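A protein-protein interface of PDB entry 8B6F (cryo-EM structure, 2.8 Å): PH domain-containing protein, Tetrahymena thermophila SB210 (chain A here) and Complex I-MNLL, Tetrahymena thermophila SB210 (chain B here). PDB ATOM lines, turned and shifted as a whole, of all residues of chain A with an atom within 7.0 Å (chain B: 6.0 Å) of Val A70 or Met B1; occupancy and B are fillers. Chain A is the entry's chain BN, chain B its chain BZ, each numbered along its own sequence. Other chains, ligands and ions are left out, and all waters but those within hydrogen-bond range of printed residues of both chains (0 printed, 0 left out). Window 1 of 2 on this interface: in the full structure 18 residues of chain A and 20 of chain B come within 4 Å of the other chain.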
ATOM      1  N   TYR A  57      -8.712   3.820  -7.159  1.00  0.00           N
ATOM      2  CA  TYR A  57      -9.716   4.671  -6.533  1.00  0.00           C
ATOM      3  C   TYR A  57     -11.099   4.031  -6.498  1.00  0.00           C
ATOM      4  O   TYR A  57     -11.786   4.128  -5.474  1.00  0.00           O
ATOM      5  CB  TYR A  57      -9.783   6.028  -7.232  1.00  0.00           C
ATOM      6  CG  TYR A  57     -10.702   6.995  -6.529  1.00  0.00           C
ATOM      7  CD1 TYR A  57     -10.257   7.748  -5.451  1.00  0.00           C
ATOM      8  CD2 TYR A  57     -12.018   7.147  -6.938  1.00  0.00           C
ATOM      9  CE1 TYR A  57     -11.098   8.627  -4.803  1.00  0.00           C
ATOM     10  CE2 TYR A  57     -12.867   8.023  -6.296  1.00  0.00           C
ATOM     11  CZ  TYR A  57     -12.401   8.763  -5.231  1.00  0.00           C
ATOM     12  OH  TYR A  57     -13.246   9.638  -4.592  1.00  0.00           O
ATOM     13  N   TRP A  60     -11.002   1.648  -3.552  1.00  0.00           N
ATOM     14  CA  TRP A  60     -11.065   2.384  -2.295  1.00  0.00           C
ATOM     15  C   TRP A  60     -12.460   2.941  -2.061  1.00  0.00           C
ATOM     16  O   TRP A  60     -12.964   2.930  -0.932  1.00  0.00           O
ATOM     17  CB  TRP A  60     -10.037   3.513  -2.290  1.00  0.00           C
ATOM     18  CG  TRP A  60     -10.354   4.590  -1.301  1.00  0.00           C
ATOM     19  CD1 TRP A  60     -10.803   5.848  -1.571  1.00  0.00           C
ATOM     20  CD2 TRP A  60     -10.251   4.498   0.125  1.00  0.00           C
ATOM     21  NE1 TRP A  60     -10.983   6.547  -0.404  1.00  0.00           N
ATOM     22  CE2 TRP A  60     -10.651   5.741   0.652  1.00  0.00           C
ATOM     23  CE3 TRP A  60      -9.858   3.486   1.005  1.00  0.00           C
ATOM     24  CZ2 TRP A  60     -10.667   5.999   2.019  1.00  0.00           C
ATOM     25  CZ3 TRP A  60      -9.875   3.743   2.362  1.00  0.00           C
ATOM     26  CH2 TRP A  60     -10.277   4.989   2.857  1.00  0.00           C
ATOM     27  N   TYR A  61     -13.098   3.431  -3.122  1.00  0.00           N
ATOM     28  CA  TYR A  61     -14.461   3.931  -3.004  1.00  0.00           C
ATOM     29  C   TYR A  61     -15.405   2.828  -2.549  1.00  0.00           C
ATOM     30  O   TYR A  61     -16.245   3.042  -1.668  1.00  0.00           O
ATOM     31  CB  TYR A  61     -14.909   4.506  -4.347  1.00  0.00           C
ATOM     32  CG  TYR A  61     -16.186   5.309  -4.297  1.00  0.00           C
ATOM     33  CD1 TYR A  61     -17.428   4.689  -4.324  1.00  0.00           C
ATOM     34  CD2 TYR A  61     -16.147   6.695  -4.252  1.00  0.00           C
ATOM     35  CE1 TYR A  61     -18.593   5.429  -4.289  1.00  0.00           C
ATOM     36  CE2 TYR A  61     -17.302   7.441  -4.218  1.00  0.00           C
ATOM     37  CZ  TYR A  61     -18.522   6.803  -4.237  1.00  0.00           C
ATOM     38  OH  TYR A  61     -19.675   7.549  -4.203  1.00  0.00           O
ATOM     39  N   LEU A  62     -15.282   1.638  -3.141  1.00  0.00           N
ATOM     40  CA  LEU A  62     -16.148   0.526  -2.760  1.00  0.00           C
ATOM     41  C   LEU A  62     -15.932   0.142  -1.302  1.00  0.00           C
ATOM     42  O   LEU A  62     -16.891  -0.053  -0.549  1.00  0.00           O
ATOM     43  CB  LEU A  62     -15.889  -0.668  -3.679  1.00  0.00           C
ATOM     44  CG  LEU A  62     -16.988  -1.733  -3.725  1.00  0.00           C
ATOM     45  CD1 LEU A  62     -18.174  -1.234  -4.526  1.00  0.00           C
ATOM     46  CD2 LEU A  62     -16.465  -3.027  -4.307  1.00  0.00           C
ATOM     47  N   ALA A  63     -14.668   0.018  -0.889  1.00  0.00           N
ATOM     48  CA  ALA A  63     -14.373  -0.357   0.490  1.00  0.00           C
ATOM     49  C   ALA A  63     -14.838   0.714   1.463  1.00  0.00           C
ATOM     50  O   ALA A  63     -15.394   0.405   2.522  1.00  0.00           O
ATOM     51  CB  ALA A  63     -12.876  -0.614   0.657  1.00  0.00           C
ATOM     52  N   LYS A  64     -14.627   1.984   1.115  1.00  0.00           N
ATOM     53  CA  LYS A  64     -15.057   3.074   1.984  1.00  0.00           C
ATOM     54  C   LYS A  64     -16.569   3.081   2.151  1.00  0.00           C
ATOM     55  O   LYS A  64     -17.075   3.263   3.262  1.00  0.00           O
ATOM     56  CB  LYS A  64     -14.574   4.406   1.415  1.00  0.00           C
ATOM     57  CG  LYS A  64     -14.932   5.620   2.252  1.00  0.00           C
ATOM     58  CD  LYS A  64     -14.517   6.897   1.542  1.00  0.00           C
ATOM     59  CE  LYS A  64     -14.830   8.124   2.375  1.00  0.00           C
ATOM     60  NZ  LYS A  64     -14.464   9.378   1.663  1.00  0.00           N
ATOM     61  N   GLY A  65     -17.306   2.884   1.059  1.00  0.00           N
ATOM     62  CA  GLY A  65     -18.753   2.805   1.164  1.00  0.00           C
ATOM     63  C   GLY A  65     -19.215   1.607   1.972  1.00  0.00           C
ATOM     64  O   GLY A  65     -20.180   1.696   2.734  1.00  0.00           O
ATOM     65  N   ALA A  66     -18.540   0.469   1.810  1.00  0.00           N
ATOM     66  CA  ALA A  66     -18.944  -0.735   2.526  1.00  0.00           C
ATOM     67  C   ALA A  66     -18.775  -0.570   4.031  1.00  0.00           C
ATOM     68  O   ALA A  66     -19.713  -0.799   4.800  1.00  0.00           O
ATOM     69  CB  ALA A  66     -18.138  -1.932   2.025  1.00  0.00           C
ATOM     70  N   ASN A  68     -18.004   2.183   5.751  1.00  0.00           N
ATOM     71  CA  ASN A  68     -18.193   3.553   6.211  1.00  0.00           C
ATOM     72  C   ASN A  68     -19.018   4.265   5.145  1.00  0.00           C
ATOM     73  O   ASN A  68     -19.398   3.672   4.131  1.00  0.00           O
ATOM     74  CB  ASN A  68     -16.856   4.254   6.464  1.00  0.00           C
ATOM     75  CG  ASN A  68     -16.993   5.452   7.384  1.00  0.00           C
ATOM     76  OD1 ASN A  68     -18.025   6.122   7.398  1.00  0.00           O
ATOM     77  ND2 ASN A  68     -15.955   5.720   8.165  1.00  0.00           N
ATOM     78  N   GLY A  69     -19.300   5.537   5.378  1.00  0.00           N
ATOM     79  CA  GLY A  69     -19.987   6.311   4.359  1.00  0.00           C
ATOM     80  C   GLY A  69     -21.413   5.834   4.160  1.00  0.00           C
ATOM     81  O   GLY A  69     -22.178   5.675   5.117  1.00  0.00           O
ATOM     82  N   VAL A  70     -21.772   5.580   2.898  1.00  0.00           N
ATOM     83  CA  VAL A  70     -23.181   5.458   2.527  1.00  0.00           C
ATOM     84  C   VAL A  70     -23.857   4.335   3.309  1.00  0.00           C
ATOM     85  O   VAL A  70     -24.915   4.533   3.917  1.00  0.00           O
ATOM     86  CB  VAL A  70     -23.324   5.275   1.004  1.00  0.00           C
ATOM     87  CG1 VAL A  70     -22.642   4.004   0.514  1.00  0.00           C
ATOM     88  CG2 VAL A  70     -24.793   5.285   0.606  1.00  0.00           C
ATOM     89  N   TRP A  71     -23.274   3.136   3.292  1.00  0.00           N
ATOM     90  CA  TRP A  71     -23.936   1.997   3.919  1.00  0.00           C
ATOM     91  C   TRP A  71     -24.161   2.234   5.407  1.00  0.00           C
ATOM     92  O   TRP A  71     -25.188   1.824   5.959  1.00  0.00           O
ATOM     93  CB  TRP A  71     -23.119   0.725   3.695  1.00  0.00           C
ATOM     94  CG  TRP A  71     -23.285   0.154   2.324  1.00  0.00           C
ATOM     95  CD1 TRP A  71     -22.506   0.402   1.235  1.00  0.00           C
ATOM     96  CD2 TRP A  71     -24.300  -0.760   1.892  1.00  0.00           C
ATOM     97  NE1 TRP A  71     -22.972  -0.300   0.152  1.00  0.00           N
ATOM     98  CE2 TRP A  71     -24.072  -1.022   0.529  1.00  0.00           C
ATOM     99  CE3 TRP A  71     -25.379  -1.381   2.527  1.00  0.00           C
ATOM    100  CZ2 TRP A  71     -24.881  -1.878  -0.212  1.00  0.00           C
ATOM    101  CZ3 TRP A  71     -26.183  -2.232   1.790  1.00  0.00           C
ATOM    102  CH2 TRP A  71     -25.930  -2.474   0.434  1.00  0.00           C
ATOM    103  N   SER A  72     -23.215   2.892   6.070  1.00  0.00           N
ATOM    104  CA  SER A  72     -23.332   3.193   7.489  1.00  0.00           C
ATOM    105  C   SER A  72     -23.974   4.544   7.771  1.00  0.00           C
ATOM    106  O   SER A  72     -24.220   4.858   8.940  1.00  0.00           O
ATOM    107  CB  SER A  72     -21.957   3.156   8.147  1.00  0.00           C
ATOM    108  OG  SER A  72     -21.038   3.922   7.401  1.00  0.00           O
ATOM    109  N   ASN A  73     -24.251   5.351   6.747  1.00  0.00           N
ATOM    110  CA  ASN A  73     -24.753   6.700   6.982  1.00  0.00           C
ATOM    111  C   ASN A  73     -26.079   6.716   7.727  1.00  0.00           C
ATOM    112  O   ASN A  73     -26.507   7.788   8.162  1.00  0.00           O
ATOM    113  CB  ASN A  73     -24.908   7.452   5.658  1.00  0.00           C
ATOM    114  CG  ASN A  73     -23.606   8.071   5.177  1.00  0.00           C
ATOM    115  OD1 ASN A  73     -22.642   8.185   5.930  1.00  0.00           O
ATOM    116  ND2 ASN A  73     -23.582   8.489   3.917  1.00  0.00           N
ATOM    117  N   ILE A  74     -26.744   5.570   7.876  1.00  0.00           N
ATOM    118  CA  ILE A  74     -27.987   5.537   8.639  1.00  0.00           C
ATOM    119  C   ILE A  74     -27.713   5.725  10.128  1.00  0.00           C
ATOM    120  O   ILE A  74     -28.477   6.396  10.830  1.00  0.00           O
ATOM    121  CB  ILE A  74     -28.752   4.227   8.362  1.00  0.00           C
ATOM    122  CG1 ILE A  74     -27.914   3.008   8.773  1.00  0.00           C
ATOM    123  CG2 ILE A  74     -29.140   4.156   6.890  1.00  0.00           C
ATOM    124  CD1 ILE A  74     -28.595   1.666   8.537  1.00  0.00           C
ATOM    125  N   HIS A  75     -26.630   5.136  10.638  1.00  0.00           N
ATOM    126  CA  HIS A  75     -26.349   5.128  12.068  1.00  0.00           C
ATOM    127  C   HIS A  75     -24.887   5.460  12.335  1.00  0.00           C
ATOM    128  O   HIS A  75     -24.005   5.000  11.593  1.00  0.00           O
ATOM    129  CB  HIS A  75     -26.673   3.759  12.666  1.00  0.00           C
ATOM    130  CG  HIS A  75     -26.914   3.779  14.144  1.00  0.00           C
ATOM    131  ND1 HIS A  75     -25.917   3.535  15.063  1.00  0.00           N
ATOM    132  CD2 HIS A  75     -28.038   4.004  14.862  1.00  0.00           C
ATOM    133  CE1 HIS A  75     -26.415   3.618  16.284  1.00  0.00           C
ATOM    134  NE2 HIS A  75     -27.701   3.900  16.189  1.00  0.00           N
ATOM    135  N   LYS A  79     -21.688  -0.989  11.116  1.00  0.00           N
ATOM    136  CA  LYS A  79     -22.718  -1.961  10.760  1.00  0.00           C
ATOM    137  C   LYS A  79     -22.546  -3.269  11.521  1.00  0.00           C
ATOM    138  O   LYS A  79     -23.533  -3.864  11.971  1.00  0.00           O
ATOM    139  CB  LYS A  79     -22.695  -2.216   9.256  1.00  0.00           C
ATOM    140  CG  LYS A  79     -22.862  -0.958   8.423  1.00  0.00           C
ATOM    141  CD  LYS A  79     -22.924  -1.272   6.936  1.00  0.00           C
ATOM    142  CE  LYS A  79     -24.221  -1.964   6.554  1.00  0.00           C
ATOM    143  NZ  LYS A  79     -25.409  -1.116   6.854  1.00  0.00           N
ATOM    144  N   MET B   1     -18.374   5.356  -0.980  1.00  0.00           N
ATOM    145  CA  MET B   1     -18.323   6.585  -0.142  1.00  0.00           C
ATOM    146  C   MET B   1     -19.733   7.007   0.261  1.00  0.00           C
ATOM    147  O   MET B   1     -20.283   6.487   1.229  1.00  0.00           O
ATOM    148  CB  MET B   1     -17.607   7.711  -0.894  1.00  0.00           C
ATOM    149  CG  MET B   1     -17.439   8.996  -0.094  1.00  0.00           C
ATOM    150  SD  MET B   1     -16.548  10.269  -1.011  1.00  0.00           S
ATOM    151  CE  MET B   1     -17.734  10.669  -2.294  1.00  0.00           C
ATOM    152  N   SER B   2     -20.323   7.936  -0.489  1.00  0.00           N
ATOM    153  CA  SER B   2     -21.630   8.486  -0.164  1.00  0.00           C
ATOM    154  C   SER B   2     -22.680   8.246  -1.234  1.00  0.00           C
ATOM    155  O   SER B   2     -23.870   8.216  -0.910  1.00  0.00           O
ATOM    156  CB  SER B   2     -21.522   9.998   0.090  1.00  0.00           C
ATOM    157  OG  SER B   2     -20.993  10.668  -1.040  1.00  0.00           O
ATOM    158  N   SER B   3     -22.281   8.071  -2.489  1.00  0.00           N
ATOM    159  CA  SER B   3     -23.221   7.888  -3.590  1.00  0.00           C
ATOM    160  C   SER B   3     -23.445   6.397  -3.796  1.00  0.00           C
ATOM    161  O   SER B   3     -22.521   5.668  -4.168  1.00  0.00           O
ATOM    162  CB  SER B   3     -22.693   8.546  -4.862  1.00  0.00           C
ATOM    163  OG  SER B   3     -23.658   8.498  -5.899  1.00  0.00           O
ATOM    164  N   MET B   4     -24.674   5.939  -3.546  1.00  0.00           N
ATOM    165  CA  MET B   4     -24.987   4.531  -3.754  1.00  0.00           C
ATOM    166  C   MET B   4     -24.922   4.158  -5.228  1.00  0.00           C
ATOM    167  O   MET B   4     -24.588   3.016  -5.560  1.00  0.00           O
ATOM    168  CB  MET B   4     -26.369   4.211  -3.185  1.00  0.00           C
ATOM    169  CG  MET B   4     -26.759   2.748  -3.302  1.00  0.00           C
ATOM    170  SD  MET B   4     -25.596   1.633  -2.492  1.00  0.00           S
ATOM    171  CE  MET B   4     -25.873   2.047  -0.774  1.00  0.00           C
ATOM    172  N   TRP B   7     -21.300   3.587  -5.864  1.00  0.00           N
ATOM    173  CA  TRP B   7     -20.912   2.346  -5.203  1.00  0.00           C
ATOM    174  C   TRP B   7     -21.378   1.136  -6.003  1.00  0.00           C
ATOM    175  O   TRP B   7     -20.625   0.172  -6.181  1.00  0.00           O
ATOM    176  CB  TRP B   7     -21.484   2.302  -3.785  1.00  0.00           C
ATOM    177  CG  TRP B   7     -20.892   1.217  -2.934  1.00  0.00           C
ATOM    178  CD1 TRP B   7     -19.840   1.335  -2.079  1.00  0.00           C
ATOM    179  CD2 TRP B   7     -21.317  -0.150  -2.862  1.00  0.00           C
ATOM    180  NE1 TRP B   7     -19.580   0.129  -1.478  1.00  0.00           N
ATOM    181  CE2 TRP B   7     -20.474  -0.800  -1.941  1.00  0.00           C
ATOM    182  CE3 TRP B   7     -22.328  -0.887  -3.488  1.00  0.00           C
ATOM    183  CZ2 TRP B   7     -20.610  -2.151  -1.629  1.00  0.00           C
ATOM    184  CZ3 TRP B   7     -22.461  -2.228  -3.176  1.00  0.00           C
ATOM    185  CH2 TRP B   7     -21.606  -2.846  -2.255  1.00  0.00           C
ATOM    186  N   ASP B  49     -31.094   0.652  -1.208  1.00  0.00           N
ATOM    187  CA  ASP B  49     -30.820   1.702  -0.236  1.00  0.00           C
ATOM    188  C   ASP B  49     -32.107   2.405   0.171  1.00  0.00           C
ATOM    189  O   ASP B  49     -32.317   2.697   1.353  1.00  0.00           O
ATOM    190  CB  ASP B  49     -29.821   2.697  -0.822  1.00  0.00           C
ATOM    191  CG  ASP B  49     -29.418   3.770   0.164  1.00  0.00           C
ATOM    192  OD1 ASP B  49     -29.817   3.679   1.342  1.00  0.00           O
ATOM    193  OD2 ASP B  49     -28.698   4.706  -0.240  1.00  0.00           O
ATOM    194  N   ARG B  52     -34.286  -0.236   2.336  1.00  0.00           N
ATOM    195  CA  ARG B  52     -33.858  -0.481   3.710  1.00  0.00           C
ATOM    196  C   ARG B  52     -34.328   0.633   4.634  1.00  0.00           C
ATOM    197  O   ARG B  52     -34.761   0.372   5.761  1.00  0.00           O
ATOM    198  CB  ARG B  52     -32.337  -0.637   3.785  1.00  0.00           C
ATOM    199  CG  ARG B  52     -31.539   0.600   3.403  1.00  0.00           C
ATOM    200  CD  ARG B  52     -30.087   0.461   3.824  1.00  0.00           C
ATOM    201  NE  ARG B  52     -29.340   1.690   3.594  1.00  0.00           N
ATOM    202  CZ  ARG B  52     -28.096   1.899   4.003  1.00  0.00           C
ATOM    203  NH1 ARG B  52     -27.430   0.982   4.683  1.00  0.00           N
ATOM    204  NH2 ARG B  52     -27.507   3.057   3.724  1.00  0.00           N
ATOM    205  N   ARG B  53     -34.249   1.884   4.179  1.00  0.00           N
ATOM    206  CA  ARG B  53     -34.699   2.991   5.013  1.00  0.00           C
ATOM    207  C   ARG B  53     -36.214   2.975   5.180  1.00  0.00           C
ATOM    208  O   ARG B  53     -36.723   3.255   6.270  1.00  0.00           O
ATOM    209  CB  ARG B  53     -34.226   4.313   4.415  1.00  0.00           C
ATOM    210  CG  ARG B  53     -32.721   4.368   4.221  1.00  0.00           C
ATOM    211  CD  ARG B  53     -32.232   5.766   3.907  1.00  0.00           C
ATOM    212  NE  ARG B  53     -30.794   5.781   3.681  1.00  0.00           N
ATOM    213  CZ  ARG B  53     -30.046   6.875   3.669  1.00  0.00           C
ATOM    214  NH1 ARG B  53     -30.568   8.071   3.882  1.00  0.00           N
ATOM    215  NH2 ARG B  53     -28.740   6.766   3.445  1.00  0.00           N
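OH of Tyr A61 touches N of Ser B2, at 3.8 Å. Tyr A61 touches Trp B7. Trp B7 touches Gly A65. O of Met B1 touches CA of Gly A69, at 3.1 Å. Ser B2 touches Val A70 (O to CG2, 3.4 Å). CE of Met B4 touches CG2 of Val A70, at 3.7 Å. Trp A71 touches Met B4. Trp B7 touches Trp A71 (CE2 to NE1, 3.3 Å). Ile A74 touches Arg B52. Arg B52 touches Lys A79.
N of Trp A71 lies close to O of Gly A65 (3.5 Å). The backbone carbonyl oxygen (O) of Gly A69 is in hydrogen-bond range of the side-chain hydroxyl (OG) of Ser A72, 3.1 Å away. The side-chain amide oxygen (OD1) of Asn A73 sits close to the backbone carbonyl oxygen (O) of Gly A69 (2.7 Å). The side-chain amino group (NZ) of Lys A79 is in hydrogen-bond range of the backbone carbonyl oxygen (O) of Trp A71 (3.1 Å). The side-chain carboxylate (OD1) of Asp B49 lies within salt-bridge range of the guanidinium group (NE) of Arg B52, 3.0 Å away. The side-chain carboxylate of Asp B49 lies within salt-bridge range of the guanidinium group of Arg B53, 3.3 Å away.
Printed residues of chain A that touch a printed residue of chain B: Tyr A61, Leu A62, Lys A64, Gly A65, Ala A66, Gly A69, Val A70, Trp A71, Ile A74 and Lys A79. Hydrophobic or aromatic side chains of chain A within 4 Å of the printed part of chain B: Tyr A61, Leu A62, Val A70, Trp A71 and Ile A74. Printed residues of chain B that touch a printed residue of chain A: Met B1, Ser B2, Ser B3, Met B4, Trp B7, Arg B52 and Arg B53. Hydrophobic or aromatic side chains of chain B within 4 Å of the printed part of chain A: Met B1, Met B4 and Trp B7. Among the printed residues, 20 pairs touch across the chains. Among the printed residues, no Asp or Glu carboxylate lies within 4 Å of a Lys or Arg side-chain nitrogen of the other chain.
Of chain B, only Met B1, Ser B2, Met B4 and Arg B52 come within 4 Å of Val A70. Met B1 touches five residues of chain A. Of the printed residues of chain B, Ile A74 touches Arg B52 and Arg B53. Of the printed residues of chain A, Arg B53 touches Ile A74. His A75 touches none of the printed residues of chain B. The nearest residue of chain B that does not touch Val A70 is Asp B49 (4.04 Å). The nearest residue of chain A that does not touch Met B1 is Asn A68 (4.1 Å).
O of Tyr A61 sits at hydrogen-bond distance from N of Met B1 (3.2 Å). The side-chain hydroxyl of Tyr A61 sits at hydrogen-bond distance from the backbone NH of Ser B3 (3.2 Å). The backbone carbonyl oxygen of Leu A62 lies within hydrogen-bond range of the indole nitrogen of Trp B7, at 2.9 Å. The side-chain amino group (NZ) of Lys A64 sits close to the side-chain sulfur (SD) of Met B1 (3.5 Å). The backbone NH of Val A70 lies within hydrogen-bond range of the backbone carbonyl oxygen of Met B1, 2.4 Å away. O of Val A70 lies within hydrogen-bond range of NH2 of Arg B52 (3.0 Å). O of Trp A71 lies within hydrogen-bond range of NH1 of Arg B52 (2.7 Å). N of Gly A65 sits close to N of Met B1 (3.4 Å). N of Ala A66 lies close to NE1 of Trp B7, at 3.5 Å.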
